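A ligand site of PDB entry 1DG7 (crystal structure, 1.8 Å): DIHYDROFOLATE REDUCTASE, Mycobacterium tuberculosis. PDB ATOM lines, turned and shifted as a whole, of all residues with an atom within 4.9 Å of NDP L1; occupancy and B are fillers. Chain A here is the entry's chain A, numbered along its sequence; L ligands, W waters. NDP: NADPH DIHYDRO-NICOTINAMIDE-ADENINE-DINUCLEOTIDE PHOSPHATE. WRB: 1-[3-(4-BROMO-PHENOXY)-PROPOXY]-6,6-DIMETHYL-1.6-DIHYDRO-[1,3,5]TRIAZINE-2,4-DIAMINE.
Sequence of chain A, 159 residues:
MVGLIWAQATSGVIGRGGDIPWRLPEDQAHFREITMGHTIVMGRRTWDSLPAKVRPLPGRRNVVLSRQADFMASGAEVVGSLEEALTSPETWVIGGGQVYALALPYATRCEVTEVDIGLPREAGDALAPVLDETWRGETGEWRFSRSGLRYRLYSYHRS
A nitrogen (NH2) of WRB L2 sits at hydrogen-bond distance from the side-chain hydroxyl (OH) of Tyr 100 (3.1 Å). The side-chain hydroxyl (OG) of Ser 66 sits at hydrogen-bond distance from an oxygen (O2X) of NDP L1, at 2.7 Å. N of Ala 7 is in hydrogen-bond range of O7N of NDP L1 (3.0 Å). O1N of NDP L1 lies within salt-bridge range of NH1 of Arg 45, 2.9 Å away. N3A of NDP L1 lies close to N of Ser 66, at 3.5 Å. An oxygen (O2X) of NDP L1 lies within hydrogen-bond range of the side-chain amide nitrogen of Gln 68 (2.8 Å). O3D of NDP L1 is in hydrogen-bond range of O of Asp 19 (3.2 Å). The backbone NH (N) of Arg 45 sits at hydrogen-bond distance from an oxygen (O5B) of NDP L1 (3.4 Å). The backbone NH (N) of Thr 46 sits at hydrogen-bond distance from an oxygen (O2A) of NDP L1 (3.1 Å). An oxygen (O3D) of NDP L1 is in hydrogen-bond range of the backbone NH (N) of Asp 19, at 3.4 Å. OG1 of Thr 46 lies within hydrogen-bond range of O2A of NDP L1 (2.6 Å). O of Ala 7 is in hydrogen-bond range of N7N of NDP L1, 2.7 Å away. The backbone carbonyl oxygen (O) of Ile 5 lies within hydrogen-bond range of a nitrogen (NH2) of WRB L2, 2.8 Å away. The guanidinium group of Arg 44 lies within salt-bridge range of an oxygen (O2X) of NDP L1 (2.9 Å). N of Gly 97 is in hydrogen-bond range of O2N of NDP L1 (3.1 Å). N of Val 99 is in hydrogen-bond range of O1A of NDP L1, at 3.2 Å. An oxygen (O2N) of NDP L1 lies within hydrogen-bond range of the backbone NH (N) of Gln 98, 2.9 Å away. The backbone carbonyl oxygen (O) of Ile 94 lies within hydrogen-bond range of a nitrogen (NH2) of WRB L2, at 2.9 Å. N of Gly 96 lies within hydrogen-bond range of O2A of NDP L1 (2.7 Å). N of Arg 44 is in hydrogen-bond range of O4B of NDP L1, 3.5 Å away. An oxygen (O3X) of NDP L1 lies within hydrogen-bond range of the backbone NH (N) of Arg 67, 2.8 Å away. The backbone carbonyl oxygen (O) of Ile 14 is in hydrogen-bond range of a nitrogen (N7N) of NDP L1.
The backbone carbonyl oxygen (O) of Ala 126 sits at hydrogen-bond distance from the backbone NH (N) of Ile 14 (3.0 Å). The side-chain hydroxyl (OG) of Ser 49 lies within hydrogen-bond range of the backbone carbonyl oxygen (O) of Thr 46 (2.7 Å). The backbone NH (N) of Gly 95 sits close to the side-chain hydroxyl (OH) of Tyr 100 (3.4 Å). The backbone carbonyl oxygen of Ile 94 is in hydrogen-bond range of the side-chain hydroxyl of Tyr 100 (3.1 Å). The side-chain amide oxygen (OE1) of Gln 98 is in hydrogen-bond range of the guanidinium group (NH1) of Arg 45, 3.2 Å away. The side-chain hydroxyl (OG) of Ser 66 sits at hydrogen-bond distance from the backbone NH (N) of Gln 68. The backbone carbonyl oxygen (O) of Leu 65 is in hydrogen-bond range of the backbone NH (N) of Arg 44, 3.0 Å away. The side-chain hydroxyl (OG1) of Thr 46 lies within hydrogen-bond range of the backbone NH (N) of Gly 96 (2.9 Å).
An oxygen (O4B) of NDP L1 lies close to the backbone carbonyl oxygen (O) of Leu 65 (3.3 Å). O of Gly 80 lies close to N1A of NDP L1, at 3.4 Å. Trp 6 touches NDP L1 (CA to O7N, 3.5 Å). Gly 15 touches NDP L1 (CA to O3D, 3.6 Å). Arg 16 touches NDP L1. Gly 18 touches NDP L1 (C to O3D, 3.4 Å). Ile 20 touches NDP L1. CA of Gly 43 touches O5B of NDP L1 (3.4 Å). Ile 94 touches NDP L1 (O to C5N, 3.3 Å). CA of Gly 95 touches C5N of NDP L1, at 3.7 Å. OH of Tyr 100 touches C4N of NDP L1, 3.4 Å away. Leu 102 touches NDP L1 (CD2 to N6A, 3.5 Å). Ala 126 touches NDP L1. Hydrophobic or aromatic side chains within 4 Å of NDP L1: Trp 6, Ile 14, Ile 20, Leu 65, Val 99, Leu 102 and Ala 126.
Water W7 lies within hydrogen-bond range of O3B of NDP L1 (2.8 Å), OE1 of Gln 98 (2.8 Å) and NH2 of Arg 45 (3.1 Å). Water W5 lies within hydrogen-bond range of NH1 of Arg 67 and O3X of NDP L1. Water W6 bridges O2D of NDP L1 (2.8 Å) and OG of Ser 49 (2.8 Å). Water W2 bridges N1A of NDP L1 (3.1 Å) and O of Gly 80 (3.5 Å).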
ATOM      1  N   ILE A   5     -19.266   3.039  11.874  1.00  0.00           N
ATOM      2  CA  ILE A   5     -19.066   1.696  12.457  1.00  0.00           C
ATOM      3  C   ILE A   5     -19.939   0.691  11.704  1.00  0.00           C
ATOM      4  O   ILE A   5     -21.122   0.932  11.472  1.00  0.00           O
ATOM      5  CB  ILE A   5     -19.336   1.645  13.999  1.00  0.00           C
ATOM      6  CG1 ILE A   5     -19.059   0.247  14.551  1.00  0.00           C
ATOM      7  CG2 ILE A   5     -20.745   2.072  14.337  1.00  0.00           C
ATOM      8  CD1 ILE A   5     -18.991   0.199  16.079  1.00  0.00           C
ATOM      9  N   TRP A   6     -19.317  -0.382  11.236  1.00  0.00           N
ATOM     10  CA  TRP A   6     -20.069  -1.388  10.494  1.00  0.00           C
ATOM     11  C   TRP A   6     -19.433  -2.779  10.564  1.00  0.00           C
ATOM     12  O   TRP A   6     -18.260  -2.916  10.953  1.00  0.00           O
ATOM     13  CB  TRP A   6     -20.205  -0.952   9.017  1.00  0.00           C
ATOM     14  CG  TRP A   6     -18.956  -1.130   8.170  1.00  0.00           C
ATOM     15  CD1 TRP A   6     -18.539  -2.286   7.553  1.00  0.00           C
ATOM     16  CD2 TRP A   6     -18.016  -0.121   7.789  1.00  0.00           C
ATOM     17  NE1 TRP A   6     -17.391  -2.061   6.831  1.00  0.00           N
ATOM     18  CE2 TRP A   6     -17.054  -0.738   6.951  1.00  0.00           C
ATOM     19  CE3 TRP A   6     -17.892   1.245   8.081  1.00  0.00           C
ATOM     20  CZ2 TRP A   6     -15.985  -0.024   6.393  1.00  0.00           C
ATOM     21  CZ3 TRP A   6     -16.824   1.949   7.525  1.00  0.00           C
ATOM     22  CH2 TRP A   6     -15.892   1.313   6.689  1.00  0.00           C
ATOM     23  N   ALA A   7     -20.223  -3.805  10.208  1.00  0.00           N
ATOM     24  CA  ALA A   7     -19.749  -5.187  10.159  1.00  0.00           C
ATOM     25  C   ALA A   7     -20.036  -5.627   8.723  1.00  0.00           C
ATOM     26  O   ALA A   7     -21.151  -5.455   8.226  1.00  0.00           O
ATOM     27  CB  ALA A   7     -20.524  -6.065  11.147  1.00  0.00           C
ATOM     28  N   ILE A  14     -23.005  -5.845   3.565  1.00  0.00           N
ATOM     29  CA  ILE A  14     -23.372  -5.491   4.921  1.00  0.00           C
ATOM     30  C   ILE A  14     -24.860  -5.707   5.150  1.00  0.00           C
ATOM     31  O   ILE A  14     -25.324  -5.757   6.292  1.00  0.00           O
ATOM     32  CB  ILE A  14     -23.031  -4.003   5.286  1.00  0.00           C
ATOM     33  CG1 ILE A  14     -23.811  -3.030   4.410  1.00  0.00           C
ATOM     34  CG2 ILE A  14     -21.539  -3.757   5.209  1.00  0.00           C
ATOM     35  CD1 ILE A  14     -23.825  -1.584   4.961  1.00  0.00           C
ATOM     36  N   GLY A  15     -25.622  -5.825   4.066  1.00  0.00           N
ATOM     37  CA  GLY A  15     -27.056  -6.025   4.160  1.00  0.00           C
ATOM     38  C   GLY A  15     -27.668  -6.643   2.918  1.00  0.00           C
ATOM     39  O   GLY A  15     -27.172  -6.429   1.801  1.00  0.00           O
ATOM     40  N   ARG A  16     -28.731  -7.427   3.105  1.00  0.00           N
ATOM     41  CA  ARG A  16     -29.439  -8.107   2.015  1.00  0.00           C
ATOM     42  C   ARG A  16     -30.871  -8.373   2.453  1.00  0.00           C
ATOM     43  O   ARG A  16     -31.088  -8.851   3.570  1.00  0.00           O
ATOM     44  CB  ARG A  16     -28.750  -9.441   1.658  1.00  0.00           C
ATOM     45  CG  ARG A  16     -29.412 -10.170   0.486  1.00  0.00           C
ATOM     46  CD  ARG A  16     -28.590 -11.356   0.050  1.00  0.00           C
ATOM     47  NE  ARG A  16     -27.309 -10.960  -0.524  1.00  0.00           N
ATOM     48  CZ  ARG A  16     -26.280 -11.787  -0.679  1.00  0.00           C
ATOM     49  NH1 ARG A  16     -26.371 -13.050  -0.304  1.00  0.00           N
ATOM     50  NH2 ARG A  16     -25.147 -11.356  -1.227  1.00  0.00           N
ATOM     51  N   GLY A  18     -33.075  -6.339   3.487  1.00  0.00           N
ATOM     52  CA  GLY A  18     -33.462  -5.587   4.674  1.00  0.00           C
ATOM     53  C   GLY A  18     -32.878  -6.096   5.979  1.00  0.00           C
ATOM     54  O   GLY A  18     -33.208  -5.595   7.046  1.00  0.00           O
ATOM     55  N   ASP A  19     -31.968  -7.076   5.886  1.00  0.00           N
ATOM     56  CA  ASP A  19     -31.340  -7.682   7.060  1.00  0.00           C
ATOM     57  C   ASP A  19     -29.835  -7.674   6.936  1.00  0.00           C
ATOM     58  O   ASP A  19     -29.270  -7.258   5.926  1.00  0.00           O
ATOM     59  CB  ASP A  19     -31.668  -9.182   7.140  1.00  0.00           C
ATOM     60  CG  ASP A  19     -33.079  -9.451   7.572  1.00  0.00           C
ATOM     61  OD1 ASP A  19     -33.787 -10.193   6.836  1.00  0.00           O
ATOM     62  OD2 ASP A  19     -33.443  -8.983   8.665  1.00  0.00           O
ATOM     63  N   ILE A  20     -29.213  -8.251   7.972  1.00  0.00           N
ATOM     64  CA  ILE A  20     -27.780  -8.459   8.046  1.00  0.00           C
ATOM     65  C   ILE A  20     -27.716  -9.986   7.864  1.00  0.00           C
ATOM     66  O   ILE A  20     -28.214 -10.745   8.703  1.00  0.00           O
ATOM     67  CB  ILE A  20     -27.213  -8.016   9.393  1.00  0.00           C
ATOM     68  CG1 ILE A  20     -27.337  -6.497   9.513  1.00  0.00           C
ATOM     69  CG2 ILE A  20     -25.763  -8.442   9.511  1.00  0.00           C
ATOM     70  CD1 ILE A  20     -26.792  -5.906  10.795  1.00  0.00           C
ATOM     71  N   TRP A  22     -26.125 -12.622   8.483  1.00  0.00           N
ATOM     72  CA  TRP A  22     -25.325 -13.446   9.399  1.00  0.00           C
ATOM     73  C   TRP A  22     -25.707 -13.136  10.842  1.00  0.00           C
ATOM     74  O   TRP A  22     -26.416 -12.164  11.124  1.00  0.00           O
ATOM     75  CB  TRP A  22     -23.814 -13.257   9.215  1.00  0.00           C
ATOM     76  CG  TRP A  22     -23.316 -11.861   9.512  1.00  0.00           C
ATOM     77  CD1 TRP A  22     -23.066 -11.317  10.745  1.00  0.00           C
ATOM     78  CD2 TRP A  22     -22.996 -10.850   8.556  1.00  0.00           C
ATOM     79  NE1 TRP A  22     -22.612 -10.030  10.610  1.00  0.00           N
ATOM     80  CE2 TRP A  22     -22.566  -9.715   9.270  1.00  0.00           C
ATOM     81  CE3 TRP A  22     -23.036 -10.792   7.159  1.00  0.00           C
ATOM     82  CZ2 TRP A  22     -22.165  -8.537   8.637  1.00  0.00           C
ATOM     83  CZ3 TRP A  22     -22.635  -9.614   6.526  1.00  0.00           C
ATOM     84  CH2 TRP A  22     -22.211  -8.498   7.278  1.00  0.00           C
ATOM     85  N   GLY A  43     -29.652   5.840   8.522  1.00  0.00           N
ATOM     86  CA  GLY A  43     -30.621   6.092   7.479  1.00  0.00           C
ATOM     87  C   GLY A  43     -31.947   5.508   7.926  1.00  0.00           C
ATOM     88  O   GLY A  43     -31.970   4.626   8.796  1.00  0.00           O
ATOM     89  N   ARG A  44     -33.031   5.976   7.335  1.00  0.00           N
ATOM     90  CA  ARG A  44     -34.374   5.512   7.695  1.00  0.00           C
ATOM     91  C   ARG A  44     -34.541   4.006   7.550  1.00  0.00           C
ATOM     92  O   ARG A  44     -35.265   3.375   8.336  1.00  0.00           O
ATOM     93  CB  ARG A  44     -35.434   6.261   6.876  1.00  0.00           C
ATOM     94  CG  ARG A  44     -36.872   6.068   7.342  1.00  0.00           C
ATOM     95  CD  ARG A  44     -37.545   4.908   6.623  1.00  0.00           C
ATOM     96  NE  ARG A  44     -37.464   5.057   5.164  1.00  0.00           N
ATOM     97  CZ  ARG A  44     -37.678   4.065   4.302  1.00  0.00           C
ATOM     98  NH1 ARG A  44     -38.023   2.860   4.730  1.00  0.00           N
ATOM     99  NH2 ARG A  44     -37.526   4.285   3.003  1.00  0.00           N
ATOM    100  N   ARG A  45     -33.914   3.417   6.535  1.00  0.00           N
ATOM    101  CA  ARG A  45     -34.035   1.981   6.352  1.00  0.00           C
ATOM    102  C   ARG A  45     -33.389   1.240   7.501  1.00  0.00           C
ATOM    103  O   ARG A  45     -33.929   0.227   7.978  1.00  0.00           O
ATOM    104  CB  ARG A  45     -33.409   1.547   5.039  1.00  0.00           C
ATOM    105  CG  ARG A  45     -34.262   1.829   3.846  1.00  0.00           C
ATOM    106  CD  ARG A  45     -33.607   1.253   2.618  1.00  0.00           C
ATOM    107  NE  ARG A  45     -34.394   1.482   1.401  1.00  0.00           N
ATOM    108  CZ  ARG A  45     -33.875   1.463   0.186  1.00  0.00           C
ATOM    109  NH1 ARG A  45     -32.582   1.233   0.017  1.00  0.00           N
ATOM    110  NH2 ARG A  45     -34.659   1.652  -0.867  1.00  0.00           N
ATOM    111  N   THR A  46     -32.230   1.707   7.962  1.00  0.00           N
ATOM    112  CA  THR A  46     -31.561   1.061   9.083  1.00  0.00           C
ATOM    113  C   THR A  46     -32.460   1.164  10.319  1.00  0.00           C
ATOM    114  O   THR A  46     -32.592   0.203  11.067  1.00  0.00           O
ATOM    115  CB  THR A  46     -30.152   1.665   9.319  1.00  0.00           C
ATOM    116  OG1 THR A  46     -29.312   1.274   8.223  1.00  0.00           O
ATOM    117  CG2 THR A  46     -29.520   1.148  10.636  1.00  0.00           C
ATOM    118  N   SER A  49     -35.061  -1.426  10.222  1.00  0.00           N
ATOM    119  CA  SER A  49     -34.504  -2.753  10.447  1.00  0.00           C
ATOM    120  C   SER A  49     -34.194  -3.077  11.898  1.00  0.00           C
ATOM    121  O   SER A  49     -33.903  -4.232  12.231  1.00  0.00           O
ATOM    122  CB  SER A  49     -33.226  -2.939   9.609  1.00  0.00           C
ATOM    123  OG  SER A  49     -32.127  -2.296  10.214  1.00  0.00           O
ATOM    124  N   LEU A  65     -31.981   9.801   9.347  1.00  0.00           N
ATOM    125  CA  LEU A  65     -31.993  10.574   8.111  1.00  0.00           C
ATOM    126  C   LEU A  65     -33.125  10.120   7.211  1.00  0.00           C
ATOM    127  O   LEU A  65     -33.173   8.958   6.811  1.00  0.00           O
ATOM    128  CB  LEU A  65     -30.685  10.357   7.341  1.00  0.00           C
ATOM    129  CG  LEU A  65     -29.608  11.439   7.325  1.00  0.00           C
ATOM    130  CD1 LEU A  65     -30.159  12.727   6.727  1.00  0.00           C
ATOM    131  CD2 LEU A  65     -29.096  11.669   8.722  1.00  0.00           C
ATOM    132  N   SER A  66     -33.983  11.051   6.838  1.00  0.00           N
ATOM    133  CA  SER A  66     -35.099  10.746   5.944  1.00  0.00           C
ATOM    134  C   SER A  66     -35.429  11.959   5.080  1.00  0.00           C
ATOM    135  O   SER A  66     -35.231  13.099   5.494  1.00  0.00           O
ATOM    136  CB  SER A  66     -36.328  10.339   6.745  1.00  0.00           C
ATOM    137  OG  SER A  66     -37.409  10.022   5.884  1.00  0.00           O
ATOM    138  N   ARG A  67     -35.880  11.712   3.861  1.00  0.00           N
ATOM    139  CA  ARG A  67     -36.283  12.800   2.961  1.00  0.00           C
ATOM    140  C   ARG A  67     -37.757  13.172   3.156  1.00  0.00           C
ATOM    141  O   ARG A  67     -38.248  14.116   2.546  1.00  0.00           O
ATOM    142  CB  ARG A  67     -36.016  12.462   1.485  1.00  0.00           C
ATOM    143  CG  ARG A  67     -34.567  12.520   1.088  1.00  0.00           C
ATOM    144  CD  ARG A  67     -34.437  12.632  -0.414  1.00  0.00           C
ATOM    145  NE  ARG A  67     -33.049  12.543  -0.848  1.00  0.00           N
ATOM    146  CZ  ARG A  67     -32.379  11.393  -1.003  1.00  0.00           C
ATOM    147  NH1 ARG A  67     -32.969  10.226  -0.740  1.00  0.00           N
ATOM    148  NH2 ARG A  67     -31.119  11.421  -1.414  1.00  0.00           N
ATOM    149  N   GLN A  68     -38.478  12.373   3.946  1.00  0.00           N
ATOM    150  CA  GLN A  68     -39.878  12.642   4.253  1.00  0.00           C
ATOM    151  C   GLN A  68     -39.848  13.571   5.477  1.00  0.00           C
ATOM    152  O   GLN A  68     -39.464  13.150   6.578  1.00  0.00           O
ATOM    153  CB  GLN A  68     -40.602  11.350   4.597  1.00  0.00           C
ATOM    154  CG  GLN A  68     -40.240  10.151   3.717  1.00  0.00           C
ATOM    155  CD  GLN A  68     -40.815   8.843   4.255  1.00  0.00           C
ATOM    156  OE1 GLN A  68     -41.955   8.811   4.732  1.00  0.00           O
ATOM    157  NE2 GLN A  68     -40.014   7.778   4.213  1.00  0.00           N
ATOM    158  N   GLY A  80     -33.659  15.936   7.890  1.00  0.00           N
ATOM    159  CA  GLY A  80     -33.737  15.759   6.447  1.00  0.00           C
ATOM    160  C   GLY A  80     -32.459  15.965   5.680  1.00  0.00           C
ATOM    161  O   GLY A  80     -32.444  15.765   4.465  1.00  0.00           O
ATOM    162  N   SER A  81     -31.398  16.379   6.355  1.00  0.00           N
ATOM    163  CA  SER A  81     -30.137  16.607   5.685  1.00  0.00           C
ATOM    164  C   SER A  81     -28.986  16.075   6.534  1.00  0.00           C
ATOM    165  O   SER A  81     -29.125  15.880   7.752  1.00  0.00           O
ATOM    166  CB  SER A  81     -29.923  18.091   5.386  1.00  0.00           C
ATOM    167  OG  SER A  81     -29.629  18.820   6.576  1.00  0.00           O
ATOM    168  N   ILE A  94     -24.070   4.680  12.030  1.00  0.00           N
ATOM    169  CA  ILE A  94     -24.270   3.253  12.183  1.00  0.00           C
ATOM    170  C   ILE A  94     -24.969   2.526  11.047  1.00  0.00           C
ATOM    171  O   ILE A  94     -25.359   1.370  11.204  1.00  0.00           O
ATOM    172  CB  ILE A  94     -25.014   2.967  13.503  1.00  0.00           C
ATOM    173  CG1 ILE A  94     -26.461   3.425  13.417  1.00  0.00           C
ATOM    174  CG2 ILE A  94     -24.305   3.685  14.644  1.00  0.00           C
ATOM    175  CD1 ILE A  94     -27.366   2.790  14.428  1.00  0.00           C
ATOM    176  N   GLY A  95     -25.135   3.091   9.960  1.00  0.00           N
ATOM    177  CA  GLY A  95     -25.612   2.533   8.690  1.00  0.00           C
ATOM    178  C   GLY A  95     -26.547   3.231   7.921  1.00  0.00           C
ATOM    179  O   GLY A  95     -27.198   4.167   8.451  1.00  0.00           O
ATOM    180  N   GLY A  96     -27.352   2.840   6.770  1.00  0.00           N
ATOM    181  CA  GLY A  96     -26.812   1.667   6.085  1.00  0.00           C
ATOM    182  C   GLY A  96     -25.860   2.031   4.959  1.00  0.00           C
ATOM    183  O   GLY A  96     -25.048   2.958   5.085  1.00  0.00           O
ATOM    184  N   GLY A  97     -25.936   1.281   3.859  1.00  0.00           N
ATOM    185  CA  GLY A  97     -25.060   1.548   2.719  1.00  0.00           C
ATOM    186  C   GLY A  97     -25.092   2.983   2.210  1.00  0.00           C
ATOM    187  O   GLY A  97     -24.045   3.596   2.014  1.00  0.00           O
ATOM    188  N   GLN A  98     -26.295   3.527   2.001  1.00  0.00           N
ATOM    189  CA  GLN A  98     -26.420   4.897   1.507  1.00  0.00           C
ATOM    190  C   GLN A  98     -25.817   5.916   2.463  1.00  0.00           C
ATOM    191  O   GLN A  98     -25.030   6.783   2.048  1.00  0.00           O
ATOM    192  CB  GLN A  98     -27.878   5.262   1.268  1.00  0.00           C
ATOM    193  CG  GLN A  98     -28.578   4.463   0.199  1.00  0.00           C
ATOM    194  CD  GLN A  98     -30.035   4.822   0.069  1.00  0.00           C
ATOM    195  OE1 GLN A  98     -30.875   3.966  -0.193  1.00  0.00           O
ATOM    196  NE2 GLN A  98     -30.354   6.087   0.293  1.00  0.00           N
ATOM    197  N   VAL A  99     -26.153   5.816   3.752  1.00  0.00           N
ATOM    198  CA  VAL A  99     -25.644   6.763   4.737  1.00  0.00           C
ATOM    199  C   VAL A  99     -24.139   6.677   4.966  1.00  0.00           C
ATOM    200  O   VAL A  99     -23.514   7.718   5.158  1.00  0.00           O
ATOM    201  CB  VAL A  99     -26.486   6.766   6.059  1.00  0.00           C
ATOM    202  CG1 VAL A  99     -25.871   7.719   7.072  1.00  0.00           C
ATOM    203  CG2 VAL A  99     -27.926   7.208   5.766  1.00  0.00           C
ATOM    204  N   TYR A 100     -23.546   5.488   4.906  1.00  0.00           N
ATOM    205  CA  TYR A 100     -22.087   5.356   5.056  1.00  0.00           C
ATOM    206  C   TYR A 100     -21.388   6.132   3.938  1.00  0.00           C
ATOM    207  O   TYR A 100     -20.439   6.879   4.171  1.00  0.00           O
ATOM    208  CB  TYR A 100     -21.636   3.901   4.974  1.00  0.00           C
ATOM    209  CG  TYR A 100     -21.927   3.055   6.211  1.00  0.00           C
ATOM    210  CD1 TYR A 100     -22.374   1.742   6.078  1.00  0.00           C
ATOM    211  CD2 TYR A 100     -21.749   3.560   7.509  1.00  0.00           C
ATOM    212  CE1 TYR A 100     -22.665   0.941   7.194  1.00  0.00           C
ATOM    213  CE2 TYR A 100     -22.033   2.751   8.639  1.00  0.00           C
ATOM    214  CZ  TYR A 100     -22.493   1.448   8.468  1.00  0.00           C
ATOM    215  OH  TYR A 100     -22.808   0.624   9.544  1.00  0.00           O
ATOM    216  N   LEU A 102     -22.593   8.560   2.185  1.00  0.00           N
ATOM    217  CA  LEU A 102     -22.909   9.971   2.371  1.00  0.00           C
ATOM    218  C   LEU A 102     -22.021  10.613   3.431  1.00  0.00           C
ATOM    219  O   LEU A 102     -21.514  11.724   3.247  1.00  0.00           O
ATOM    220  CB  LEU A 102     -24.366  10.090   2.793  1.00  0.00           C
ATOM    221  CG  LEU A 102     -25.202  11.337   2.489  1.00  0.00           C
ATOM    222  CD1 LEU A 102     -25.256  11.610   0.974  1.00  0.00           C
ATOM    223  CD2 LEU A 102     -26.628  11.135   3.057  1.00  0.00           C
ATOM    224  N   ALA A 126     -26.674  -4.102   0.254  1.00  0.00           N
ATOM    225  CA  ALA A 126     -26.183  -2.895   0.902  1.00  0.00           C
ATOM    226  C   ALA A 126     -24.702  -3.241   1.010  1.00  0.00           C
ATOM    227  O   ALA A 126     -24.339  -4.401   1.338  1.00  0.00           O
ATOM    228  CB  ALA A 126     -26.817  -2.730   2.294  1.00  0.00           C
HETATM  229  PA  NDP L   1     -29.994   3.318   4.757  1.00  0.00           P
HETATM  230  O1A NDP L   1     -28.703   3.977   4.440  1.00  0.00           O
HETATM  231  O2A NDP L   1     -30.013   2.753   6.142  1.00  0.00           O
HETATM  232  O5B NDP L   1     -31.240   4.340   4.615  1.00  0.00           O
HETATM  233  C5B NDP L   1     -31.460   4.982   3.309  1.00  0.00           C
HETATM  234  C4B NDP L   1     -32.552   6.051   3.618  1.00  0.00           C
HETATM  235  O4B NDP L   1     -31.901   7.176   4.291  1.00  0.00           O
HETATM  236  C3B NDP L   1     -33.153   6.601   2.467  1.00  0.00           C
HETATM  237  O3B NDP L   1     -34.109   5.686   1.947  1.00  0.00           O
HETATM  238  C2B NDP L   1     -33.701   7.963   3.055  1.00  0.00           C
HETATM  239  O2B NDP L   1     -34.854   7.877   3.848  1.00  0.00           O
HETATM  240  C1B NDP L   1     -32.528   8.390   3.844  1.00  0.00           C
HETATM  241  N9A NDP L   1     -31.590   9.192   3.092  1.00  0.00           N
HETATM  242  C8A NDP L   1     -30.559   8.798   2.299  1.00  0.00           C
HETATM  243  N7A NDP L   1     -29.872   9.808   1.797  1.00  0.00           N
HETATM  244  C5A NDP L   1     -30.503  10.897   2.311  1.00  0.00           C
HETATM  245  C6A NDP L   1     -30.240  12.319   2.149  1.00  0.00           C
HETATM  246  N6A NDP L   1     -29.219  12.731   1.373  1.00  0.00           N
HETATM  247  N1A NDP L   1     -31.083  13.175   2.800  1.00  0.00           N
HETATM  248  C2A NDP L   1     -32.109  12.652   3.559  1.00  0.00           C
HETATM  249  N3A NDP L   1     -32.414  11.393   3.766  1.00  0.00           N
HETATM  250  C4A NDP L   1     -31.551  10.556   3.112  1.00  0.00           C
HETATM  251  O3  NDP L   1     -30.312   2.239   3.745  1.00  0.00           O
HETATM  252  PN  NDP L   1     -29.667   1.081   2.924  1.00  0.00           P
HETATM  253  O1N NDP L   1     -30.679   0.423   2.060  1.00  0.00           O
HETATM  254  O2N NDP L   1     -28.485   1.563   2.153  1.00  0.00           O
HETATM  255  O5D NDP L   1     -29.098   0.062   4.087  1.00  0.00           O
HETATM  256  C5D NDP L   1     -30.066  -0.732   4.830  1.00  0.00           C
HETATM  257  C4D NDP L   1     -29.425  -2.132   4.872  1.00  0.00           C
HETATM  258  O4D NDP L   1     -28.178  -2.065   5.569  1.00  0.00           O
HETATM  259  C3D NDP L   1     -30.277  -3.190   5.628  1.00  0.00           C
HETATM  260  O3D NDP L   1     -30.156  -4.399   4.911  1.00  0.00           O
HETATM  261  C2D NDP L   1     -29.596  -3.212   7.012  1.00  0.00           C
HETATM  262  O2D NDP L   1     -29.888  -4.451   7.664  1.00  0.00           O
HETATM  263  C1D NDP L   1     -28.138  -3.059   6.617  1.00  0.00           C
HETATM  264  N1N NDP L   1     -27.243  -2.534   7.707  1.00  0.00           N
HETATM  265  C2N NDP L   1     -26.058  -3.275   7.926  1.00  0.00           C
HETATM  266  C3N NDP L   1     -25.200  -2.782   8.880  1.00  0.00           C
HETATM  267  C7N NDP L   1     -23.895  -3.574   9.117  1.00  0.00           C
HETATM  268  O7N NDP L   1     -23.051  -3.044   9.800  1.00  0.00           O
HETATM  269  N7N NDP L   1     -23.788  -4.812   8.535  1.00  0.00           N
HETATM  270  C4N NDP L   1     -25.415  -1.606   9.677  1.00  0.00           C
HETATM  271  C5N NDP L   1     -26.660  -0.974   9.345  1.00  0.00           C
HETATM  272  C6N NDP L   1     -27.555  -1.372   8.416  1.00  0.00           C
HETATM  273  P2B NDP L   1     -36.370   7.981   3.097  1.00  0.00           P
HETATM  274  O1X NDP L   1     -36.446   6.875   2.160  1.00  0.00           O
HETATM  275  O2X NDP L   1     -37.208   7.848   4.359  1.00  0.00           O
HETATM  276  O3X NDP L   1     -36.303   9.342   2.502  1.00  0.00           O
HETATM  277  C1  WRB L   2     -23.885  -3.674  13.809  1.00  0.00           C
HETATM  278  N2  WRB L   2     -22.580  -3.899  14.327  1.00  0.00           N
HETATM  279  C3  WRB L   2     -21.590  -3.079  13.858  1.00  0.00           C
HETATM  280  N4  WRB L   2     -21.903  -1.862  13.359  1.00  0.00           N
HETATM  281  C5  WRB L   2     -23.158  -1.572  13.011  1.00  0.00           C
HETATM  282  N6  WRB L   2     -24.149  -2.243  13.645  1.00  0.00           N
HETATM  283  O7  WRB L   2     -25.422  -2.039  13.001  1.00  0.00           O
HETATM  284  C8  WRB L   2     -26.200  -1.074  13.734  1.00  0.00           C
HETATM  285  C9  WRB L   2     -27.659  -1.123  13.259  1.00  0.00           C
HETATM  286  C10 WRB L   2     -28.336  -2.424  13.680  1.00  0.00           C
HETATM  287  O11 WRB L   2     -27.853  -2.729  15.016  1.00  0.00           O
HETATM  288  C12 WRB L   2     -28.748  -3.550  15.813  1.00  0.00           C
HETATM  289  C13 WRB L   2     -29.491  -4.600  15.195  1.00  0.00           C
HETATM  290  C14 WRB L   2     -30.112  -5.564  16.069  1.00  0.00           C
HETATM  291  C15 WRB L   2     -28.611  -3.410  17.215  1.00  0.00           C
HETATM  292  C16 WRB L   2     -29.230  -4.358  18.073  1.00  0.00           C
HETATM  293  C17 WRB L   2     -29.994  -5.449  17.519  1.00  0.00           C
HETATM  294  CM1 WRB L   2     -24.876  -4.215  14.774  1.00  0.00           C
HETATM  295  CM2 WRB L   2     -24.060  -4.406  12.524  1.00  0.00           C
HETATM  296  NH1 WRB L   2     -20.317  -3.325  14.215  1.00  0.00           N
HETATM  297  NH2 WRB L   2     -23.400  -0.366  12.455  1.00  0.00           N
HETATM  298 BR   WRB L   2     -30.891  -6.694  18.726  1.00  0.00          BR
HETATM  299  O   HOH W   1     -38.494   9.865   1.156  1.00  0.00           O
HETATM  300  O   HOH W   2     -29.836  15.923   2.201  1.00  0.00           O
HETATM  301  O   HOH W   3     -27.389  15.619   2.065  1.00  0.00           O
HETATM  302  O   HOH W   4     -28.097   9.650  -0.085  1.00  0.00           O
HETATM  303  O   HOH W   5     -35.445   9.370  -0.134  1.00  0.00           O
HETATM  304  O   HOH W   6     -29.702  -3.746  10.341  1.00  0.00           O
HETATM  305  O   HOH W   7     -33.630   4.577  -0.537  1.00  0.00           O
